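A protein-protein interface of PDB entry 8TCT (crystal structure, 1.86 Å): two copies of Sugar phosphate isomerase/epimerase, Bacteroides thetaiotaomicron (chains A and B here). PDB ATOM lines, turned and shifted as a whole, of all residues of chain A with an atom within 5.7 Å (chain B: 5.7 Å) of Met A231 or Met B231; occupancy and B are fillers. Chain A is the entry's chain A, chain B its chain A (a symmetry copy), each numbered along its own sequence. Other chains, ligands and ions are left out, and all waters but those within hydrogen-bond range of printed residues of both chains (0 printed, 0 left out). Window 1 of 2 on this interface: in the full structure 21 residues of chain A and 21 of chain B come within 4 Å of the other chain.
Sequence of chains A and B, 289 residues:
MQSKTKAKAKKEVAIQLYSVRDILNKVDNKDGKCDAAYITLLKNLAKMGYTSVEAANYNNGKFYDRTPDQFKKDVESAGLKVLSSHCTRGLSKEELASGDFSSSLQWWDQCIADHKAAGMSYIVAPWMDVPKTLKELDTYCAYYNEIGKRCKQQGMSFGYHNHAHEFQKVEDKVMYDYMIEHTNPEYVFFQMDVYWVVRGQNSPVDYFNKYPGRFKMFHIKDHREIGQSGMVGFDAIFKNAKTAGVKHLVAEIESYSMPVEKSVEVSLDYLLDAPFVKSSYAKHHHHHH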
ATOM      1  N   TYR A 195     -12.922  10.931 -30.400  1.00  0.00           N
ATOM      2  CA  TYR A 195     -11.723  10.157 -30.163  1.00  0.00           C
ATOM      3  C   TYR A 195     -11.454  10.032 -28.694  1.00  0.00           C
ATOM      4  O   TYR A 195     -11.267   8.908 -28.220  1.00  0.00           O
ATOM      5  CB  TYR A 195     -10.481  10.797 -30.753  1.00  0.00           C
ATOM      6  CG  TYR A 195      -9.148  10.131 -30.442  1.00  0.00           C
ATOM      7  CD1 TYR A 195      -8.766   8.949 -31.080  1.00  0.00           C
ATOM      8  CD2 TYR A 195      -8.255  10.715 -29.574  1.00  0.00           C
ATOM      9  CE1 TYR A 195      -7.520   8.372 -30.837  1.00  0.00           C
ATOM     10  CE2 TYR A 195      -7.026  10.129 -29.306  1.00  0.00           C
ATOM     11  CZ  TYR A 195      -6.660   8.960 -29.952  1.00  0.00           C
ATOM     12  OH  TYR A 195      -5.453   8.422 -29.704  1.00  0.00           O
ATOM     13  N   VAL A 198     -13.971   7.818 -26.745  1.00  0.00           N
ATOM     14  CA  VAL A 198     -13.626   6.421 -26.916  1.00  0.00           C
ATOM     15  C   VAL A 198     -12.368   6.054 -26.120  1.00  0.00           C
ATOM     16  O   VAL A 198     -12.371   5.092 -25.352  1.00  0.00           O
ATOM     17  CB  VAL A 198     -13.504   6.138 -28.410  1.00  0.00           C
ATOM     18  CG1 VAL A 198     -13.055   4.699 -28.674  1.00  0.00           C
ATOM     19  CG2 VAL A 198     -14.801   6.399 -29.118  1.00  0.00           C
ATOM     20  N   ARG A 199     -11.314   6.863 -26.184  1.00  0.00           N
ATOM     21  CA  ARG A 199     -10.170   6.659 -25.313  1.00  0.00           C
ATOM     22  C   ARG A 199     -10.592   6.608 -23.852  1.00  0.00           C
ATOM     23  O   ARG A 199      -9.960   5.897 -23.067  1.00  0.00           O
ATOM     24  CB  ARG A 199      -9.057   7.722 -25.433  1.00  0.00           C
ATOM     25  CG  ARG A 199      -8.412   7.770 -26.817  1.00  0.00           C
ATOM     26  CD  ARG A 199      -7.499   6.647 -27.158  1.00  0.00           C
ATOM     27  NE  ARG A 199      -6.402   6.618 -26.184  1.00  0.00           N
ATOM     28  CZ  ARG A 199      -5.263   7.312 -26.123  1.00  0.00           C
ATOM     29  NH1 ARG A 199      -4.539   7.171 -25.039  1.00  0.00           N
ATOM     30  NH2 ARG A 199      -4.827   8.122 -27.085  1.00  0.00           N
ATOM     31  N   GLN A 201     -13.164   5.319 -22.720  1.00  0.00           N
ATOM     32  CA  GLN A 201     -13.880   4.065 -22.517  1.00  0.00           C
ATOM     33  C   GLN A 201     -15.375   4.271 -22.613  1.00  0.00           C
ATOM     34  O   GLN A 201     -16.101   3.541 -21.963  1.00  0.00           O
ATOM     35  CB  GLN A 201     -13.592   3.413 -21.155  1.00  0.00           C
ATOM     36  CG  GLN A 201     -12.119   3.401 -20.764  1.00  0.00           C
ATOM     37  CD  GLN A 201     -11.349   2.415 -21.624  1.00  0.00           C
ATOM     38  OE1 GLN A 201     -11.372   1.210 -21.384  1.00  0.00           O
ATOM     39  NE2 GLN A 201     -10.722   2.897 -22.679  1.00  0.00           N
ATOM     40  N   ASN A 202     -15.841   5.234 -23.415  1.00  0.00           N
ATOM     41  CA  ASN A 202     -17.262   5.533 -23.426  1.00  0.00           C
ATOM     42  C   ASN A 202     -17.720   5.573 -24.851  1.00  0.00           C
ATOM     43  O   ASN A 202     -16.907   5.582 -25.779  1.00  0.00           O
ATOM     44  CB  ASN A 202     -17.549   6.821 -22.662  1.00  0.00           C
ATOM     45  CG  ASN A 202     -17.755   6.562 -21.197  1.00  0.00           C
ATOM     46  OD1 ASN A 202     -18.890   6.344 -20.785  1.00  0.00           O
ATOM     47  ND2 ASN A 202     -16.720   6.671 -20.417  1.00  0.00           N
ATOM     48  N   SER A 203     -19.043   5.617 -24.991  1.00  0.00           N
ATOM     49  CA  SER A 203     -19.723   5.507 -26.270  1.00  0.00           C
ATOM     50  C   SER A 203     -20.223   6.895 -26.657  1.00  0.00           C
ATOM     51  O   SER A 203     -21.136   7.412 -25.979  1.00  0.00           O
ATOM     52  CB  SER A 203     -20.915   4.563 -26.208  1.00  0.00           C
ATOM     53  OG  SER A 203     -21.751   4.693 -27.362  1.00  0.00           O
ATOM     54  N   PRO A 204     -19.718   7.485 -27.763  1.00  0.00           N
ATOM     55  CA  PRO A 204     -20.298   8.707 -28.292  1.00  0.00           C
ATOM     56  C   PRO A 204     -21.786   8.593 -28.515  1.00  0.00           C
ATOM     57  O   PRO A 204     -22.519   9.484 -28.121  1.00  0.00           O
ATOM     58  CB  PRO A 204     -19.547   8.939 -29.585  1.00  0.00           C
ATOM     59  CG  PRO A 204     -18.164   8.343 -29.285  1.00  0.00           C
ATOM     60  CD  PRO A 204     -18.465   7.114 -28.466  1.00  0.00           C
ATOM     61  N   ASP A 222      -8.320  11.406 -34.593  1.00  0.00           N
ATOM     62  CA  ASP A 222      -7.973   9.986 -34.529  1.00  0.00           C
ATOM     63  C   ASP A 222      -6.581   9.954 -33.953  1.00  0.00           C
ATOM     64  O   ASP A 222      -6.071  10.974 -33.480  1.00  0.00           O
ATOM     65  CB  ASP A 222      -8.211   9.318 -35.873  1.00  0.00           C
ATOM     66  CG  ASP A 222      -8.413   7.804 -35.848  1.00  0.00           C
ATOM     67  OD1 ASP A 222      -8.056   7.190 -34.817  1.00  0.00           O
ATOM     68  OD2 ASP A 222      -8.919   7.317 -36.863  1.00  0.00           O
ATOM     69  N   HIS A 223      -6.033   8.752 -33.865  1.00  0.00           N
ATOM     70  CA  HIS A 223      -4.727   8.532 -33.285  1.00  0.00           C
ATOM     71  C   HIS A 223      -3.656   9.282 -34.092  1.00  0.00           C
ATOM     72  O   HIS A 223      -2.820   9.982 -33.536  1.00  0.00           O
ATOM     73  CB  HIS A 223      -4.513   7.012 -33.223  1.00  0.00           C
ATOM     74  CG  HIS A 223      -3.280   6.603 -32.575  1.00  0.00           C
ATOM     75  ND1 HIS A 223      -2.946   6.948 -31.287  1.00  0.00           N
ATOM     76  CD2 HIS A 223      -2.289   5.814 -33.038  1.00  0.00           C
ATOM     77  CE1 HIS A 223      -1.762   6.404 -30.982  1.00  0.00           C
ATOM     78  NE2 HIS A 223      -1.357   5.718 -32.028  1.00  0.00           N
ATOM     79  N   SER A 229      -6.938   4.563 -37.874  1.00  0.00           N
ATOM     80  CA  SER A 229      -6.387   3.759 -36.805  1.00  0.00           C
ATOM     81  C   SER A 229      -7.214   2.495 -36.503  1.00  0.00           C
ATOM     82  O   SER A 229      -6.674   1.580 -35.899  1.00  0.00           O
ATOM     83  CB  SER A 229      -6.273   4.540 -35.561  1.00  0.00           C
ATOM     84  OG  SER A 229      -7.588   4.786 -35.065  1.00  0.00           O
ATOM     85  N   GLY A 230      -8.529   2.518 -36.770  1.00  0.00           N
ATOM     86  CA  GLY A 230      -9.478   1.536 -36.245  1.00  0.00           C
ATOM     87  C   GLY A 230     -10.051   1.897 -34.868  1.00  0.00           C
ATOM     88  O   GLY A 230     -10.818   1.120 -34.293  1.00  0.00           O
ATOM     89  N   MET A 231      -9.646   3.046 -34.298  1.00  0.00           N
ATOM     90  CA  MET A 231      -9.944   3.360 -32.925  1.00  0.00           C
ATOM     91  C   MET A 231     -11.246   4.189 -32.775  1.00  0.00           C
ATOM     92  O   MET A 231     -11.651   4.397 -31.654  1.00  0.00           O
ATOM     93  CB  MET A 231      -8.792   4.071 -32.218  1.00  0.00           C
ATOM     94  CG  MET A 231      -7.517   3.258 -32.240  1.00  0.00           C
ATOM     95  SD  MET A 231      -6.139   4.138 -31.507  1.00  0.00           S
ATOM     96  CE  MET A 231      -6.529   4.199 -29.757  1.00  0.00           C
ATOM     97  N   VAL A 232     -11.901   4.611 -33.854  1.00  0.00           N
ATOM     98  CA  VAL A 232     -13.063   5.478 -33.701  1.00  0.00           C
ATOM     99  C   VAL A 232     -14.084   5.022 -34.698  1.00  0.00           C
ATOM    100  O   VAL A 232     -13.815   4.959 -35.901  1.00  0.00           O
ATOM    101  CB  VAL A 232     -12.761   6.983 -33.889  1.00  0.00           C
ATOM    102  CG1 VAL A 232     -13.970   7.866 -33.537  1.00  0.00           C
ATOM    103  CG2 VAL A 232     -11.605   7.420 -33.019  1.00  0.00           C
ATOM    104  N   GLY A 233     -15.273   4.693 -34.170  1.00  0.00           N
ATOM    105  CA  GLY A 233     -16.380   4.284 -35.024  1.00  0.00           C
ATOM    106  C   GLY A 233     -17.123   5.472 -35.631  1.00  0.00           C
ATOM    107  O   GLY A 233     -18.309   5.687 -35.342  1.00  0.00           O
ATOM    108  N   TYR B 195     -12.254  -4.629 -30.575  1.00  0.00           N
ATOM    109  CA  TYR B 195     -12.882  -3.845 -29.534  1.00  0.00           C
ATOM    110  C   TYR B 195     -11.969  -3.699 -28.355  1.00  0.00           C
ATOM    111  O   TYR B 195     -11.747  -2.567 -27.914  1.00  0.00           O
ATOM    112  CB  TYR B 195     -14.147  -4.485 -28.994  1.00  0.00           C
ATOM    113  CG  TYR B 195     -14.809  -3.808 -27.803  1.00  0.00           C
ATOM    114  CD1 TYR B 195     -15.546  -2.632 -27.960  1.00  0.00           C
ATOM    115  CD2 TYR B 195     -14.755  -4.375 -26.551  1.00  0.00           C
ATOM    116  CE1 TYR B 195     -16.201  -2.044 -26.878  1.00  0.00           C
ATOM    117  CE2 TYR B 195     -15.380  -3.777 -25.465  1.00  0.00           C
ATOM    118  CZ  TYR B 195     -16.112  -2.615 -25.640  1.00  0.00           C
ATOM    119  OH  TYR B 195     -16.736  -2.067 -24.582  1.00  0.00           O
ATOM    120  N   VAL B 198      -8.850  -1.474 -28.957  1.00  0.00           N
ATOM    121  CA  VAL B 198      -9.217  -0.077 -28.833  1.00  0.00           C
ATOM    122  C   VAL B 198      -9.466   0.307 -27.370  1.00  0.00           C
ATOM    123  O   VAL B 198      -8.897   1.279 -26.872  1.00  0.00           O
ATOM    124  CB  VAL B 198     -10.412   0.186 -29.744  1.00  0.00           C
ATOM    125  CG1 VAL B 198     -10.917   1.625 -29.604  1.00  0.00           C
ATOM    126  CG2 VAL B 198     -10.072  -0.091 -31.178  1.00  0.00           C
ATOM    127  N   ARG B 199     -10.212  -0.496 -26.617  1.00  0.00           N
ATOM    128  CA  ARG B 199     -10.329  -0.274 -25.187  1.00  0.00           C
ATOM    129  C   ARG B 199      -8.959  -0.206 -24.527  1.00  0.00           C
ATOM    130  O   ARG B 199      -8.802   0.520 -23.541  1.00  0.00           O
ATOM    131  CB  ARG B 199     -11.155  -1.331 -24.424  1.00  0.00           C
ATOM    132  CG  ARG B 199     -12.615  -1.394 -24.867  1.00  0.00           C
ATOM    133  CD  ARG B 199     -13.485  -0.270 -24.430  1.00  0.00           C
ATOM    134  NE  ARG B 199     -13.493  -0.222 -22.963  1.00  0.00           N
ATOM    135  CZ  ARG B 199     -14.204  -0.908 -22.065  1.00  0.00           C
ATOM    136  NH1 ARG B 199     -13.881  -0.749 -20.805  1.00  0.00           N
ATOM    137  NH2 ARG B 199     -15.206  -1.728 -22.372  1.00  0.00           N
ATOM    138  N   GLN B 201      -6.407   1.083 -25.702  1.00  0.00           N
ATOM    139  CA  GLN B 201      -5.785   2.336 -26.117  1.00  0.00           C
ATOM    140  C   GLN B 201      -4.858   2.119 -27.292  1.00  0.00           C
ATOM    141  O   GLN B 201      -3.894   2.853 -27.408  1.00  0.00           O
ATOM    142  CB  GLN B 201      -4.968   3.007 -25.003  1.00  0.00           C
ATOM    143  CG  GLN B 201      -5.660   3.033 -23.644  1.00  0.00           C
ATOM    144  CD  GLN B 201      -6.820   4.012 -23.659  1.00  0.00           C
ATOM    145  OE1 GLN B 201      -6.633   5.220 -23.532  1.00  0.00           O
ATOM    146  NE2 GLN B 201      -8.021   3.520 -23.890  1.00  0.00           N
ATOM    147  N   ASN B 202      -5.138   1.143 -28.161  1.00  0.00           N
ATOM    148  CA  ASN B 202      -4.196   0.835 -29.222  1.00  0.00           C
ATOM    149  C   ASN B 202      -4.951   0.774 -30.514  1.00  0.00           C
ATOM    150  O   ASN B 202      -6.185   0.757 -30.528  1.00  0.00           O
ATOM    151  CB  ASN B 202      -3.428  -0.444 -28.909  1.00  0.00           C
ATOM    152  CG  ASN B 202      -2.202  -0.167 -28.088  1.00  0.00           C
ATOM    153  OD1 ASN B 202      -1.138   0.050 -28.661  1.00  0.00           O
ATOM    154  ND2 ASN B 202      -2.311  -0.260 -26.796  1.00  0.00           N
ATOM    155  N   SER B 203      -4.172   0.720 -31.592  1.00  0.00           N
ATOM    156  CA  SER B 203      -4.671   0.809 -32.954  1.00  0.00           C
ATOM    157  C   SER B 203      -4.617  -0.587 -33.566  1.00  0.00           C
ATOM    158  O   SER B 203      -3.499  -1.100 -33.786  1.00  0.00           O
ATOM    159  CB  SER B 203      -3.835   1.747 -33.812  1.00  0.00           C
ATOM    160  OG  SER B 203      -4.135   1.596 -35.202  1.00  0.00           O
ATOM    161  N   PRO B 204      -5.774  -1.189 -33.920  1.00  0.00           N
ATOM    162  CA  PRO B 204      -5.774  -2.421 -34.688  1.00  0.00           C
ATOM    163  C   PRO B 204      -4.946  -2.319 -35.947  1.00  0.00           C
ATOM    164  O   PRO B 204      -4.159  -3.209 -36.218  1.00  0.00           O
ATOM    165  CB  PRO B 204      -7.236  -2.665 -34.990  1.00  0.00           C
ATOM    166  CG  PRO B 204      -7.940  -2.057 -33.767  1.00  0.00           C
ATOM    167  CD  PRO B 204      -7.136  -0.820 -33.461  1.00  0.00           C
ATOM    168  N   ASP B 222     -18.445  -5.132 -29.940  1.00  0.00           N
ATOM    169  CA  ASP B 222     -18.637  -3.709 -29.659  1.00  0.00           C
ATOM    170  C   ASP B 222     -19.138  -3.662 -28.238  1.00  0.00           C
ATOM    171  O   ASP B 222     -19.120  -4.672 -27.528  1.00  0.00           O
ATOM    172  CB  ASP B 222     -19.483  -3.061 -30.741  1.00  0.00           C
ATOM    173  CG  ASP B 222     -19.338  -1.548 -30.895  1.00  0.00           C
ATOM    174  OD1 ASP B 222     -18.813  -0.919 -29.949  1.00  0.00           O
ATOM    175  OD2 ASP B 222     -19.759  -1.077 -31.956  1.00  0.00           O
ATOM    176  N   HIS B 223     -19.446  -2.456 -27.787  1.00  0.00           N
ATOM    177  CA  HIS B 223     -19.886  -2.220 -26.430  1.00  0.00           C
ATOM    178  C   HIS B 223     -21.197  -2.975 -26.162  1.00  0.00           C
ATOM    179  O   HIS B 223     -21.338  -3.661 -25.159  1.00  0.00           O
ATOM    180  CB  HIS B 223     -19.992  -0.698 -26.250  1.00  0.00           C
ATOM    181  CG  HIS B 223     -20.336  -0.273 -24.905  1.00  0.00           C
ATOM    182  ND1 HIS B 223     -19.597  -0.599 -23.792  1.00  0.00           N
ATOM    183  CD2 HIS B 223     -21.346   0.515 -24.487  1.00  0.00           C
ATOM    184  CE1 HIS B 223     -20.164  -0.044 -22.714  1.00  0.00           C
ATOM    185  NE2 HIS B 223     -21.217   0.631 -23.120  1.00  0.00           N
ATOM    186  N   SER B 229     -21.851   1.674 -31.193  1.00  0.00           N
ATOM    187  CA  SER B 229     -21.427   2.496 -30.080  1.00  0.00           C
ATOM    188  C   SER B 229     -20.658   3.759 -30.511  1.00  0.00           C
ATOM    189  O   SER B 229     -20.574   4.685 -29.717  1.00  0.00           O
ATOM    190  CB  SER B 229     -20.573   1.732 -29.154  1.00  0.00           C
ATOM    191  OG  SER B 229     -19.324   1.485 -29.798  1.00  0.00           O
ATOM    192  N   GLY B 230     -19.978   3.724 -31.667  1.00  0.00           N
ATOM    193  CA  GLY B 230     -18.960   4.708 -32.037  1.00  0.00           C
ATOM    194  C   GLY B 230     -17.550   4.362 -31.539  1.00  0.00           C
ATOM    195  O   GLY B 230     -16.615   5.142 -31.737  1.00  0.00           O
ATOM    196  N   MET B 231     -17.389   3.223 -30.842  1.00  0.00           N
ATOM    197  CA  MET B 231     -16.166   2.925 -30.143  1.00  0.00           C
ATOM    198  C   MET B 231     -15.181   2.090 -31.001  1.00  0.00           C
ATOM    199  O   MET B 231     -14.074   1.895 -30.552  1.00  0.00           O
ATOM    200  CB  MET B 231     -16.406   2.231 -28.804  1.00  0.00           C
ATOM    201  CG  MET B 231     -17.277   3.051 -27.881  1.00  0.00           C
ATOM    202  SD  MET B 231     -17.646   2.189 -26.353  1.00  0.00           S
ATOM    203  CE  MET B 231     -16.083   2.149 -25.475  1.00  0.00           C
ATOM    204  N   VAL B 232     -15.545   1.651 -32.203  1.00  0.00           N
ATOM    205  CA  VAL B 232     -14.650   0.779 -32.955  1.00  0.00           C
ATOM    206  C   VAL B 232     -14.713   1.215 -34.387  1.00  0.00           C
ATOM    207  O   VAL B 232     -15.788   1.264 -34.990  1.00  0.00           O
ATOM    208  CB  VAL B 232     -14.982  -0.727 -32.835  1.00  0.00           C
ATOM    209  CG1 VAL B 232     -13.908  -1.612 -33.490  1.00  0.00           C
ATOM    210  CG2 VAL B 232     -15.104  -1.145 -31.389  1.00  0.00           C
ATOM    211  N   GLY B 233     -13.528   1.544 -34.924  1.00  0.00           N
ATOM    212  CA  GLY B 233     -13.428   1.935 -36.324  1.00  0.00           C
ATOM    213  C   GLY B 233     -13.376   0.735 -37.266  1.00  0.00           C
ATOM    214  O   GLY B 233     -12.368   0.517 -37.953  1.00  0.00           O
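Asn A202 touches Met B231, and with the chains exchanged Met A231 touches Asn B202. Gly A230 touches Val B232, and with the chains exchanged Val A232 touches Gly B230. Gly A230 touches Gly B233, and with the chains exchanged Gly A233 touches Gly B230. Met B231 touches its own counterpart, Met A231. Positions printed for both chains: 195, 198, 199, 201, 202, 203, 204, 222, 223, 229, 230, 231, 232 and 233. Of the 27 pairs that touch across the chains among the printed residues, 27 have their exchanged pair printed and touching as well.
Hydrophobic or aromatic side chains of chain A that line the printed part of chain B: Val A198, Pro A204 and Met A231. Of the 14 printed residues of chain B, 11 touch a printed residue of chain A. Among the printed residues, no Asp or Glu carboxylate lies within 4 Å of a Lys or Arg side-chain nitrogen of the other chain.
OH of Tyr A195 is in hydrogen-bond range of NH2 of Arg A199 (2.7 Å). The side-chain amide nitrogen (NE2) of Gln A201 sits at hydrogen-bond distance from the backbone carbonyl oxygen (O) of Arg A199. The side-chain carboxylate (OD1) of Asp A222 is in hydrogen-bond range of the side-chain hydroxyl (OG) of Ser A229. The guanidinium group (NH2) of Arg B199 lies within hydrogen-bond range of the side-chain hydroxyl (OH) of Tyr B195, at 2.7 Å. The backbone carbonyl oxygen of Arg B199 lies within hydrogen-bond range of the side-chain amide nitrogen of Gln B201. The side-chain carboxylate (OD1) of Asp B222 sits at hydrogen-bond distance from the side-chain hydroxyl (OG) of Ser B229 (2.5 Å).
Among the printed residues, merely in contact across the chains: Val A198 with Val B198 (3.9 Å), Val A198 with Gly B230 (3.4 Å), Val A198 with Met B231 (3.5 Å), Gln A201 with Met B231 (3.6 Å), Ser A203 with Met B231 (3.8 Å), Pro A204 with Ser B229 (3.5 Å), Ser A229 with Pro B204 (3.5 Å), Gly A230 with Val B198 (3.4 Å), Gly A230 with Val B232 (3.9 Å), Met A231 with Val B198 (3.5 Å), Met A231 with Gln B201 (3.6 Å), Met A231 with Ser B203 (3.8 Å), Met A231 with Met B231 (3.7 Å), Val A232 with Gly B230 (3.9 Å), Val A232 with Val B232 (3.9 Å), Val A232 with Gly B233 (3.1 Å), Gly A233 with Val B232 (3.1 Å) and Gly A233 with Gly B233 (3.7 Å).
Met A231 touches just these residues of chain B: Val B198 (3.5 Å), Gln B201 (3.6 Å), Asn B202 (3.3 Å), Ser B203 (3.8 Å) and Met B231 (3.7 Å). Met B231 touches five residues of chain A. Printed residues of chain A within 4 Å of Ser B229: Ser A203 (2.6 Å) and Pro A204 (3.5 Å). Of the printed residues of chain B, Val A232 touches Gly B230, Val B232 and Gly B233. Of the printed residues of chain A, Ser B203 touches Ser A229 and Met A231. Printed residues of chain B within 4 Å of Gln A201: Arg B199, Gln B201 and Met B231. His B223 touches none of the printed residues of chain A. Asp A222 touches none of the printed residues of chain B. The nearest residue of chain B that does not touch Met A231 is Gly B233 (4.1 Å). The nearest printed residue of chain A that does not touch Gln B201 is Val A198 (4.9 Å).
OE1 of Gln B201 sits at hydrogen-bond distance from NE of Arg A199, 3.0 Å away. NE of Arg B199 lies within hydrogen-bond range of OE1 of Gln A201 (3.0 Å). The side-chain amide nitrogen (NE2) of Gln A201 sits close to the side-chain amide nitrogen (NE2) of Gln B201 (3.0 Å). The side-chain hydroxyl (OG) of Ser A203 lies within hydrogen-bond range of the backbone carbonyl oxygen (O) of Ser B229. The backbone carbonyl oxygen (O) of Ser A229 is in hydrogen-bond range of the side-chain hydroxyl (OG) of Ser B203. N of Gly B233 lies within hydrogen-bond range of O of Gly A230. N of Gly A233 is in hydrogen-bond range of O of Gly B230. O of Asn A202 lies close to SD of Met B231, 3.5 Å away. SD of Met A231 sits close to O of Asn B202.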
